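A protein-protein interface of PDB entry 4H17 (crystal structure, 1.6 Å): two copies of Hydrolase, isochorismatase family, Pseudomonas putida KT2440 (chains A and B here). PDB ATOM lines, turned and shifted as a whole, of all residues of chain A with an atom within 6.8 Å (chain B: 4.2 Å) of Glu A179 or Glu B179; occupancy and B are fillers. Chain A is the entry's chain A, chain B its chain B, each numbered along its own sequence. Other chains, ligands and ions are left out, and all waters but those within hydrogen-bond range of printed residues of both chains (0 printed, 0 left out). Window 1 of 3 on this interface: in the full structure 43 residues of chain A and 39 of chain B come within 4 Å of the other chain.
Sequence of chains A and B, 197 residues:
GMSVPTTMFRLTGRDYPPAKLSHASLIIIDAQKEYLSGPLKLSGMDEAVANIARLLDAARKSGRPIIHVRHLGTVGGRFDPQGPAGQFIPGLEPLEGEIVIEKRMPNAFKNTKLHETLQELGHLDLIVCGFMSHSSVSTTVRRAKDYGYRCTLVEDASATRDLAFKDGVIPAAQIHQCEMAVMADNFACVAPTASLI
Among the printed residues, pairs that only touch across the chains: His A134 with Val B182 (3.5 Å), Ser A135 with Arg B142 (3.5 Å), Ile A170 with Gln B177 (3.9 Å), Ile A170 with Cys B178 (3.97 Å), Ile A170 with Ala B181 (3.8 Å) and Gln A174 with Cys B178 (3.96 Å).
The backbone NH of Ser A138 sits at hydrogen-bond distance from the backbone carbonyl oxygen of Ser A133, at 3.0 Å. OE2 of Glu A179 lies within salt-bridge range of NH2 of Arg A142 (3.1 Å). The guanidinium group of Arg B142 is in hydrogen-bond range of the side-chain hydroxyl of Ser B138 (2.9 Å). OG of Ser A138 is in hydrogen-bond range of OE2 of Glu A179, 2.8 Å away. The side-chain hydroxyl (OG) of Ser B138 is in hydrogen-bond range of the side-chain carboxylate (OE2) of Glu B179 (2.8 Å). The side-chain hydroxyl of Thr A139 is in hydrogen-bond range of the backbone carbonyl oxygen of Ser A135 (2.7 Å).
Arg A142 touches its own counterpart, Arg B142. Arg A142 touches Glu B179, and with the chains exchanged Glu A179 touches Arg B142. Cys A178 touches its own counterpart, Cys B178. Glu A179 touches its own counterpart, Glu B179. 11 positions are printed for both chains. Of the 15 pairs that touch across the chains among the printed residues, 7 have their exchanged pair printed and touching as well.
Of chain A, only Arg A142 (3.6 Å) and Glu A179 (2.5 Å) come within 4 Å of Glu B179. Printed residues of chain B within 4 Å of Gln A174: Cys B178. Of the printed residues of chain B, Ile A170 touches Gln B177 (3.9 Å), Cys B178 (3.97 Å) and Ala B181 (3.8 Å). Printed residues of chain B within 4 Å of Arg A142: Ser B138, Arg B142 and Glu B179. Met B183 touches none of the printed residues of chain A. The nearest residue of chain A that does not touch Glu B179 is Val A182 (4.5 Å). The nearest printed residue of chain B that does not touch Gln A174 is Gln B177 (6.6 Å).
NE of Arg A142 sits close to NE of Arg B142, 3.4 Å away. SG of Cys B178 sits at hydrogen-bond distance from SG of Cys A178 (3.3 Å). The side-chain hydroxyl (OG1) of Thr A139 lies within hydrogen-bond range of the guanidinium group (NH1) of Arg B142 (2.9 Å). The guanidinium group (NH2) of Arg B142 lies close to the side-chain hydroxyl (OG) of Ser A138, at 3.4 Å. The side-chain hydroxyl (OG) of Ser B138 is in hydrogen-bond range of the guanidinium group (NH2) of Arg A142 (3.5 Å). The side-chain carboxylate of Glu B179 sits close to the side-chain carboxylate of Glu A179. O of His A134 sits at hydrogen-bond distance from NH1 of Arg B142 (2.9 Å). The side-chain carboxylate (OE2) of Glu A179 is in salt-bridge range of the guanidinium group (NH2) of Arg B142. The guanidinium group (NH2) of Arg A142 is in salt-bridge range of the side-chain carboxylate (OE2) of Glu B179, 3.6 Å away.
Of the 21 printed residues of chain A, 9 touch a printed residue of chain B. Hydrophobic or aromatic side chains of chain A that line the printed part of chain B: His A134 and Ile A170. Hydrophobic or aromatic side chains of chain B that line the printed part of chain A: Ala B181 and Val B182. Among the printed residues, 15 pairs touch across the chains. Among the printed residues, Asp or Glu carboxylates within 4 Å of a Lys or Arg side-chain nitrogen of the other chain: Arg A142 with Glu B179 (3.6 Å) and Glu A179 with Arg B142 (3.5 Å).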
ATOM      1  N   SER A 133      15.365  23.772 -22.846  1.00  0.00           N
ATOM      2  CA  SER A 133      14.435  23.857 -21.727  1.00  0.00           C
ATOM      3  C   SER A 133      14.250  25.303 -21.277  1.00  0.00           C
ATOM      4  O   SER A 133      13.124  25.689 -20.942  1.00  0.00           O
ATOM      5  CB  SER A 133      14.873  22.973 -20.553  1.00  0.00           C
ATOM      6  OG  SER A 133      16.142  23.274 -20.106  1.00  0.00           O
ATOM      7  N   HIS A 134      15.318  26.092 -21.236  1.00  0.00           N
ATOM      8  CA  HIS A 134      15.272  27.455 -20.649  1.00  0.00           C
ATOM      9  C   HIS A 134      14.739  28.513 -21.625  1.00  0.00           C
ATOM     10  O   HIS A 134      14.479  29.646 -21.230  1.00  0.00           O
ATOM     11  CB  HIS A 134      16.631  27.906 -20.113  1.00  0.00           C
ATOM     12  CG  HIS A 134      17.649  28.101 -21.177  1.00  0.00           C
ATOM     13  ND1 HIS A 134      18.251  27.049 -21.823  1.00  0.00           N
ATOM     14  CD2 HIS A 134      18.123  29.221 -21.767  1.00  0.00           C
ATOM     15  CE1 HIS A 134      19.051  27.505 -22.764  1.00  0.00           C
ATOM     16  NE2 HIS A 134      19.026  28.820 -22.722  1.00  0.00           N
ATOM     17  N   SER A 135      14.663  28.169 -22.910  1.00  0.00           N
ATOM     18  CA  SER A 135      14.411  29.157 -23.964  1.00  0.00           C
ATOM     19  C   SER A 135      13.067  28.887 -24.659  1.00  0.00           C
ATOM     20  O   SER A 135      12.042  29.299 -24.149  1.00  0.00           O
ATOM     21  CB  SER A 135      15.611  29.256 -24.919  1.00  0.00           C
ATOM     22  OG  SER A 135      15.350  30.159 -25.966  1.00  0.00           O
ATOM     23  N   SER A 138      10.497  26.807 -22.000  1.00  0.00           N
ATOM     24  CA  SER A 138      10.055  27.710 -20.936  1.00  0.00           C
ATOM     25  C   SER A 138       9.126  28.786 -21.476  1.00  0.00           C
ATOM     26  O   SER A 138       8.021  29.030 -20.907  1.00  0.00           O
ATOM     27  CB  SER A 138      11.264  28.350 -20.240  1.00  0.00           C
ATOM     28  OG  SER A 138      10.780  29.189 -19.202  1.00  0.00           O
ATOM     29  N   THR A 139       9.497  29.398 -22.597  1.00  0.00           N
ATOM     30  CA  THR A 139       8.701  30.495 -23.145  1.00  0.00           C
ATOM     31  C   THR A 139       7.337  29.999 -23.610  1.00  0.00           C
ATOM     32  O   THR A 139       6.310  30.617 -23.309  1.00  0.00           O
ATOM     33  CB  THR A 139       9.410  31.187 -24.273  1.00  0.00           C
ATOM     34  OG1 THR A 139      10.695  31.594 -23.843  1.00  0.00           O
ATOM     35  CG2 THR A 139       8.601  32.376 -24.760  1.00  0.00           C
ATOM     36  N   ARG A 142       5.112  29.037 -20.680  1.00  0.00           N
ATOM     37  CA  ARG A 142       4.595  30.261 -20.040  1.00  0.00           C
ATOM     38  C   ARG A 142       3.443  30.870 -20.849  1.00  0.00           C
ATOM     39  O   ARG A 142       2.407  31.223 -20.279  1.00  0.00           O
ATOM     40  CB  ARG A 142       5.705  31.292 -19.850  1.00  0.00           C
ATOM     41  CG  ARG A 142       6.814  30.859 -18.856  1.00  0.00           C
ATOM     42  CD  ARG A 142       8.040  31.741 -18.925  1.00  0.00           C
ATOM     43  NE  ARG A 142       9.151  31.280 -18.075  1.00  0.00           N
ATOM     44  CZ  ARG A 142       9.383  31.714 -16.836  1.00  0.00           C
ATOM     45  NH1 ARG A 142       8.627  32.643 -16.285  1.00  0.00           N
ATOM     46  NH2 ARG A 142      10.426  31.232 -16.146  1.00  0.00           N
ATOM     47  N   LEU A 153       5.201  19.235 -18.181  1.00  0.00           N
ATOM     48  CA  LEU A 153       6.492  19.324 -18.852  1.00  0.00           C
ATOM     49  C   LEU A 153       7.299  18.111 -18.505  1.00  0.00           C
ATOM     50  O   LEU A 153       7.494  17.800 -17.327  1.00  0.00           O
ATOM     51  CB  LEU A 153       7.205  20.596 -18.385  1.00  0.00           C
ATOM     52  CG  LEU A 153       8.607  20.883 -18.884  1.00  0.00           C
ATOM     53  CD1 LEU A 153       8.761  20.903 -20.381  1.00  0.00           C
ATOM     54  CD2 LEU A 153       9.050  22.205 -18.293  1.00  0.00           C
ATOM     55  N   ILE A 170      27.793  28.003 -15.867  1.00  0.00           N
ATOM     56  CA  ILE A 170      26.834  27.215 -15.094  1.00  0.00           C
ATOM     57  C   ILE A 170      26.534  25.944 -15.897  1.00  0.00           C
ATOM     58  O   ILE A 170      26.079  26.012 -17.056  1.00  0.00           O
ATOM     59  CB  ILE A 170      25.536  27.967 -14.810  1.00  0.00           C
ATOM     60  CG1 ILE A 170      25.803  29.277 -14.040  1.00  0.00           C
ATOM     61  CG2 ILE A 170      24.584  27.059 -14.018  1.00  0.00           C
ATOM     62  CD1 ILE A 170      24.652  30.234 -13.905  1.00  0.00           C
ATOM     63  N   GLN A 174      22.499  22.228 -13.933  1.00  0.00           N
ATOM     64  CA  GLN A 174      22.106  23.203 -12.905  1.00  0.00           C
ATOM     65  C   GLN A 174      21.068  24.132 -13.540  1.00  0.00           C
ATOM     66  O   GLN A 174      20.008  24.408 -12.957  1.00  0.00           O
ATOM     67  CB  GLN A 174      23.280  23.974 -12.376  1.00  0.00           C
ATOM     68  CG  GLN A 174      24.094  23.178 -11.401  1.00  0.00           C
ATOM     69  CD  GLN A 174      25.260  23.950 -10.873  1.00  0.00           C
ATOM     70  OE1 GLN A 174      25.148  25.141 -10.576  1.00  0.00           O
ATOM     71  NE2 GLN A 174      26.393  23.263 -10.709  1.00  0.00           N
ATOM     72  N   ILE A 175      21.342  24.562 -14.770  1.00  0.00           N
ATOM     73  CA  ILE A 175      20.326  25.344 -15.482  1.00  0.00           C
ATOM     74  C   ILE A 175      19.003  24.580 -15.582  1.00  0.00           C
ATOM     75  O   ILE A 175      17.948  25.125 -15.368  1.00  0.00           O
ATOM     76  CB  ILE A 175      20.770  25.695 -16.915  1.00  0.00           C
ATOM     77  CG1 ILE A 175      22.045  26.542 -16.921  1.00  0.00           C
ATOM     78  CG2 ILE A 175      19.617  26.358 -17.658  1.00  0.00           C
ATOM     79  CD1 ILE A 175      21.985  27.876 -16.209  1.00  0.00           C
ATOM     80  N   HIS A 176      19.080  23.325 -16.004  1.00  0.00           N
ATOM     81  CA  HIS A 176      17.893  22.533 -16.229  1.00  0.00           C
ATOM     82  C   HIS A 176      17.084  22.306 -14.912  1.00  0.00           C
ATOM     83  O   HIS A 176      15.884  22.477 -14.889  1.00  0.00           O
ATOM     84  CB  HIS A 176      18.273  21.240 -16.918  1.00  0.00           C
ATOM     85  CG  HIS A 176      17.102  20.478 -17.448  1.00  0.00           C
ATOM     86  ND1 HIS A 176      16.344  20.927 -18.501  1.00  0.00           N
ATOM     87  CD2 HIS A 176      16.560  19.295 -17.073  1.00  0.00           C
ATOM     88  CE1 HIS A 176      15.393  20.055 -18.767  1.00  0.00           C
ATOM     89  NE2 HIS A 176      15.511  19.047 -17.922  1.00  0.00           N
ATOM     90  N   GLN A 177      17.770  21.977 -13.836  1.00  0.00           N
ATOM     91  CA  GLN A 177      17.129  21.765 -12.533  1.00  0.00           C
ATOM     92  C   GLN A 177      16.478  23.044 -12.053  1.00  0.00           C
ATOM     93  O   GLN A 177      15.365  23.017 -11.582  1.00  0.00           O
ATOM     94  CB  GLN A 177      18.119  21.270 -11.479  1.00  0.00           C
ATOM     95  N   CYS A 178      17.180  24.170 -12.188  1.00  0.00           N
ATOM     96  CA  CYS A 178      16.580  25.428 -11.786  1.00  0.00           C
ATOM     97  C   CYS A 178      15.337  25.721 -12.616  1.00  0.00           C
ATOM     98  O   CYS A 178      14.288  26.103 -12.080  1.00  0.00           O
ATOM     99  CB  CYS A 178      17.617  26.559 -11.845  1.00  0.00           C
ATOM    100  SG  CYS A 178      18.925  26.448 -10.563  1.00  0.00           S
ATOM    101  N   GLU A 179      15.394  25.526 -13.932  1.00  0.00           N
ATOM    102  CA  GLU A 179      14.222  25.810 -14.743  1.00  0.00           C
ATOM    103  C   GLU A 179      13.072  24.860 -14.465  1.00  0.00           C
ATOM    104  O   GLU A 179      11.938  25.293 -14.509  1.00  0.00           O
ATOM    105  CB  GLU A 179      14.512  25.929 -16.218  1.00  0.00           C
ATOM    106  CG  GLU A 179      13.447  26.837 -16.936  1.00  0.00           C
ATOM    107  CD  GLU A 179      13.475  28.353 -16.612  1.00  0.00           C
ATOM    108  OE1 GLU A 179      14.404  28.838 -15.915  1.00  0.00           O
ATOM    109  OE2 GLU A 179      12.543  29.105 -17.050  1.00  0.00           O
ATOM    110  N   MET A 180      13.368  23.614 -14.085  1.00  0.00           N
ATOM    111  CA  MET A 180      12.327  22.651 -13.738  1.00  0.00           C
ATOM    112  C   MET A 180      11.678  23.096 -12.439  1.00  0.00           C
ATOM    113  O   MET A 180      10.453  23.048 -12.327  1.00  0.00           O
ATOM    114  CB  MET A 180      12.775  21.182 -13.635  1.00  0.00           C
ATOM    115  CG  MET A 180      13.217  20.465 -14.932  1.00  0.00           C
ATOM    116  SD  MET A 180      11.979  20.737 -16.409  1.00  0.00           S
ATOM    117  CE  MET A 180      12.878  22.197 -17.308  1.00  0.00           C
ATOM    118  N   ALA A 181      12.461  23.594 -11.493  1.00  0.00           N
ATOM    119  CA  ALA A 181      11.922  24.116 -10.232  1.00  0.00           C
ATOM    120  C   ALA A 181      11.017  25.339 -10.486  1.00  0.00           C
ATOM    121  O   ALA A 181       9.938  25.474  -9.879  1.00  0.00           O
ATOM    122  CB  ALA A 181      13.044  24.444  -9.249  1.00  0.00           C
ATOM    123  N   VAL A 182      11.485  26.220 -11.364  1.00  0.00           N
ATOM    124  CA  VAL A 182      10.762  27.447 -11.776  1.00  0.00           C
ATOM    125  C   VAL A 182       9.422  27.096 -12.451  1.00  0.00           C
ATOM    126  O   VAL A 182       8.368  27.629 -12.106  1.00  0.00           O
ATOM    127  CB  VAL A 182      11.670  28.307 -12.693  1.00  0.00           C
ATOM    128  CG1 VAL A 182      10.887  29.315 -13.528  1.00  0.00           C
ATOM    129  CG2 VAL A 182      12.771  28.965 -11.869  1.00  0.00           C
ATOM    130  N   MET A 183       9.470  26.165 -13.404  1.00  0.00           N
ATOM    131  CA  MET A 183       8.258  25.647 -14.042  1.00  0.00           C
ATOM    132  C   MET A 183       7.290  25.055 -13.036  1.00  0.00           C
ATOM    133  O   MET A 183       6.119  25.383 -13.055  1.00  0.00           O
ATOM    134  CB  MET A 183       8.662  24.588 -15.089  1.00  0.00           C
ATOM    135  CG  MET A 183       9.446  25.220 -16.255  1.00  0.00           C
ATOM    136  SD  MET A 183       8.290  26.198 -17.443  1.00  0.00           S
ATOM    137  CE  MET A 183       8.820  27.980 -16.955  1.00  0.00           C
ATOM    138  N   ALA A 184       7.779  24.190 -12.138  1.00  0.00           N
ATOM    139  CA  ALA A 184       6.936  23.529 -11.151  1.00  0.00           C
ATOM    140  C   ALA A 184       6.309  24.531 -10.175  1.00  0.00           C
ATOM    141  O   ALA A 184       5.251  24.265  -9.592  1.00  0.00           O
ATOM    142  CB  ALA A 184       7.734  22.490 -10.386  1.00  0.00           C
ATOM    143  N   ASP A 185       6.952  25.655  -9.965  1.00  0.00           N
ATOM    144  CA  ASP A 185       6.425  26.650  -9.024  1.00  0.00           C
ATOM    145  C   ASP A 185       5.102  27.248  -9.513  1.00  0.00           C
ATOM    146  O   ASP A 185       4.212  27.510  -8.697  1.00  0.00           O
ATOM    147  CB  ASP A 185       7.472  27.757  -8.818  1.00  0.00           C
ATOM    148  CG  ASP A 185       7.078  28.761  -7.759  1.00  0.00           C
ATOM    149  OD1 ASP A 185       6.545  28.311  -6.728  1.00  0.00           O
ATOM    150  OD2 ASP A 185       7.423  29.966  -7.959  1.00  0.00           O
ATOM    151  N   VAL A 190       5.550  19.139 -13.513  1.00  0.00           N
ATOM    152  CA  VAL A 190       6.792  18.595 -14.054  1.00  0.00           C
ATOM    153  C   VAL A 190       6.815  17.136 -13.676  1.00  0.00           C
ATOM    154  O   VAL A 190       6.622  16.787 -12.493  1.00  0.00           O
ATOM    155  CB  VAL A 190       8.011  19.370 -13.519  1.00  0.00           C
ATOM    156  CG1 VAL A 190       9.319  18.779 -13.998  1.00  0.00           C
ATOM    157  CG2 VAL A 190       7.926  20.859 -13.918  1.00  0.00           C
ATOM    158  N   SER B 138      10.769  37.347 -15.528  1.00  0.00           N
ATOM    159  CA  SER B 138      11.165  36.434 -16.650  1.00  0.00           C
ATOM    160  C   SER B 138      10.065  36.346 -17.699  1.00  0.00           C
ATOM    161  O   SER B 138      10.313  36.537 -18.903  1.00  0.00           O
ATOM    162  CB  SER B 138      11.506  35.044 -16.120  1.00  0.00           C
ATOM    163  OG  SER B 138      11.888  34.214 -17.195  1.00  0.00           O
ATOM    164  N   ARG B 142      10.348  37.854 -21.491  1.00  0.00           N
ATOM    165  CA  ARG B 142      10.143  36.933 -22.619  1.00  0.00           C
ATOM    166  C   ARG B 142       9.059  37.437 -23.584  1.00  0.00           C
ATOM    167  O   ARG B 142       9.237  37.395 -24.781  1.00  0.00           O
ATOM    168  CB  ARG B 142       9.868  35.506 -22.157  1.00  0.00           C
ATOM    169  CG  ARG B 142      10.988  34.879 -21.341  1.00  0.00           C
ATOM    170  CD  ARG B 142      10.502  33.626 -20.647  1.00  0.00           C
ATOM    171  NE  ARG B 142      11.540  33.009 -19.818  1.00  0.00           N
ATOM    172  CZ  ARG B 142      12.342  32.029 -20.206  1.00  0.00           C
ATOM    173  NH1 ARG B 142      12.275  31.566 -21.451  1.00  0.00           N
ATOM    174  NH2 ARG B 142      13.250  31.565 -19.368  1.00  0.00           N
ATOM    175  N   ILE B 175      18.728  30.044  -7.946  1.00  0.00           N
ATOM    176  CA  ILE B 175      17.628  30.336  -8.885  1.00  0.00           C
ATOM    177  C   ILE B 175      17.964  31.625  -9.634  1.00  0.00           C
ATOM    178  O   ILE B 175      17.817  31.681 -10.850  1.00  0.00           O
ATOM    179  CB  ILE B 175      16.256  30.470  -8.195  1.00  0.00           C
ATOM    180  CG1 ILE B 175      15.848  29.155  -7.540  1.00  0.00           C
ATOM    181  CG2 ILE B 175      15.171  30.927  -9.182  1.00  0.00           C
ATOM    182  CD1 ILE B 175      15.718  27.913  -8.418  1.00  0.00           C
ATOM    183  N   HIS B 176      18.284  32.667  -8.888  1.00  0.00           N
ATOM    184  CA  HIS B 176      18.484  33.974  -9.470  1.00  0.00           C
ATOM    185  C   HIS B 176      19.648  33.978 -10.457  1.00  0.00           C
ATOM    186  O   HIS B 176      19.505  34.472 -11.592  1.00  0.00           O
ATOM    187  CB  HIS B 176      18.654  35.002  -8.365  1.00  0.00           C
ATOM    188  CG  HIS B 176      18.535  36.419  -8.847  1.00  0.00           C
ATOM    189  ND1 HIS B 176      17.349  36.946  -9.315  1.00  0.00           N
ATOM    190  CD2 HIS B 176      19.456  37.398  -8.962  1.00  0.00           C
ATOM    191  CE1 HIS B 176      17.551  38.203  -9.671  1.00  0.00           C
ATOM    192  NE2 HIS B 176      18.815  38.496  -9.466  1.00  0.00           N
ATOM    193  N   GLN B 177      20.786  33.416 -10.071  1.00  0.00           N
ATOM    194  CA  GLN B 177      21.939  33.357 -10.961  1.00  0.00           C
ATOM    195  C   GLN B 177      21.622  32.578 -12.234  1.00  0.00           C
ATOM    196  O   GLN B 177      21.963  32.983 -13.320  1.00  0.00           O
ATOM    197  CB  GLN B 177      23.134  32.771 -10.242  1.00  0.00           C
ATOM    198  CG  GLN B 177      24.437  33.058 -10.943  1.00  0.00           C
ATOM    199  CD  GLN B 177      25.618  32.713 -10.080  1.00  0.00           C
ATOM    200  OE1 GLN B 177      26.175  31.654 -10.218  1.00  0.00           O
ATOM    201  NE2 GLN B 177      25.970  33.594  -9.168  1.00  0.00           N
ATOM    202  N   CYS B 178      20.987  31.412 -12.078  1.00  0.00           N
ATOM    203  CA  CYS B 178      20.620  30.631 -13.259  1.00  0.00           C
ATOM    204  C   CYS B 178      19.672  31.417 -14.153  1.00  0.00           C
ATOM    205  O   CYS B 178      19.839  31.458 -15.387  1.00  0.00           O
ATOM    206  CB  CYS B 178      20.004  29.286 -12.862  1.00  0.00           C
ATOM    207  SG  CYS B 178      21.224  28.089 -12.172  1.00  0.00           S
ATOM    208  N   GLU B 179      18.650  32.058 -13.575  1.00  0.00           N
ATOM    209  CA  GLU B 179      17.769  32.816 -14.423  1.00  0.00           C
ATOM    210  C   GLU B 179      18.474  34.008 -15.097  1.00  0.00           C
ATOM    211  O   GLU B 179      18.112  34.348 -16.230  1.00  0.00           O
ATOM    212  CB  GLU B 179      16.453  33.256 -13.763  1.00  0.00           C
ATOM    213  CG  GLU B 179      15.292  33.494 -14.782  1.00  0.00           C
ATOM    214  CD  GLU B 179      14.699  32.238 -15.466  1.00  0.00           C
ATOM    215  OE1 GLU B 179      15.066  31.097 -15.108  1.00  0.00           O
ATOM    216  OE2 GLU B 179      13.845  32.376 -16.406  1.00  0.00           O
ATOM    217  N   MET B 180      19.477  34.600 -14.461  1.00  0.00           N
ATOM    218  CA  MET B 180      20.248  35.683 -15.100  1.00  0.00           C
ATOM    219  C   MET B 180      21.034  35.135 -16.284  1.00  0.00           C
ATOM    220  O   MET B 180      21.082  35.773 -17.331  1.00  0.00           O
ATOM    221  CB  MET B 180      21.159  36.440 -14.145  1.00  0.00           C
ATOM    222  CG  MET B 180      20.490  37.278 -13.039  1.00  0.00           C
ATOM    223  SD  MET B 180      19.079  38.417 -13.665  1.00  0.00           S
ATOM    224  CE  MET B 180      17.522  37.323 -13.186  1.00  0.00           C
ATOM    225  N   ALA B 181      21.600  33.941 -16.147  1.00  0.00           N
ATOM    226  CA  ALA B 181      22.329  33.293 -17.265  1.00  0.00           C
ATOM    227  C   ALA B 181      21.342  32.987 -18.433  1.00  0.00           C
ATOM    228  O   ALA B 181      21.646  33.221 -19.660  1.00  0.00           O
ATOM    229  CB  ALA B 181      23.019  32.027 -16.782  1.00  0.00           C
ATOM    230  N   VAL B 182      20.170  32.478 -18.075  1.00  0.00           N
ATOM    231  CA  VAL B 182      19.074  32.213 -19.033  1.00  0.00           C
ATOM    232  C   VAL B 182      18.620  33.472 -19.793  1.00  0.00           C
ATOM    233  O   VAL B 182      18.492  33.502 -21.015  1.00  0.00           O
ATOM    234  CB  VAL B 182      17.903  31.536 -18.260  1.00  0.00           C
ATOM    235  CG1 VAL B 182      16.588  31.572 -19.049  1.00  0.00           C
ATOM    236  CG2 VAL B 182      18.270  30.121 -17.909  1.00  0.00           C
ATOM    237  N   MET B 183      18.365  34.545 -19.034  1.00  0.00           N
ATOM    238  CA  MET B 183      18.002  35.836 -19.601  1.00  0.00           C
ATOM    239  C   MET B 183      19.064  36.363 -20.538  1.00  0.00           C
ATOM    240  O   MET B 183      18.797  36.729 -21.665  1.00  0.00           O
ATOM    241  CB  MET B 183      17.716  36.827 -18.469  1.00  0.00           C
ATOM    242  CG  MET B 183      16.450  36.497 -17.657  1.00  0.00           C
ATOM    243  SD  MET B 183      14.840  36.952 -18.646  1.00  0.00           S
ATOM    244  CE  MET B 183      14.308  35.162 -19.100  1.00  0.00           C
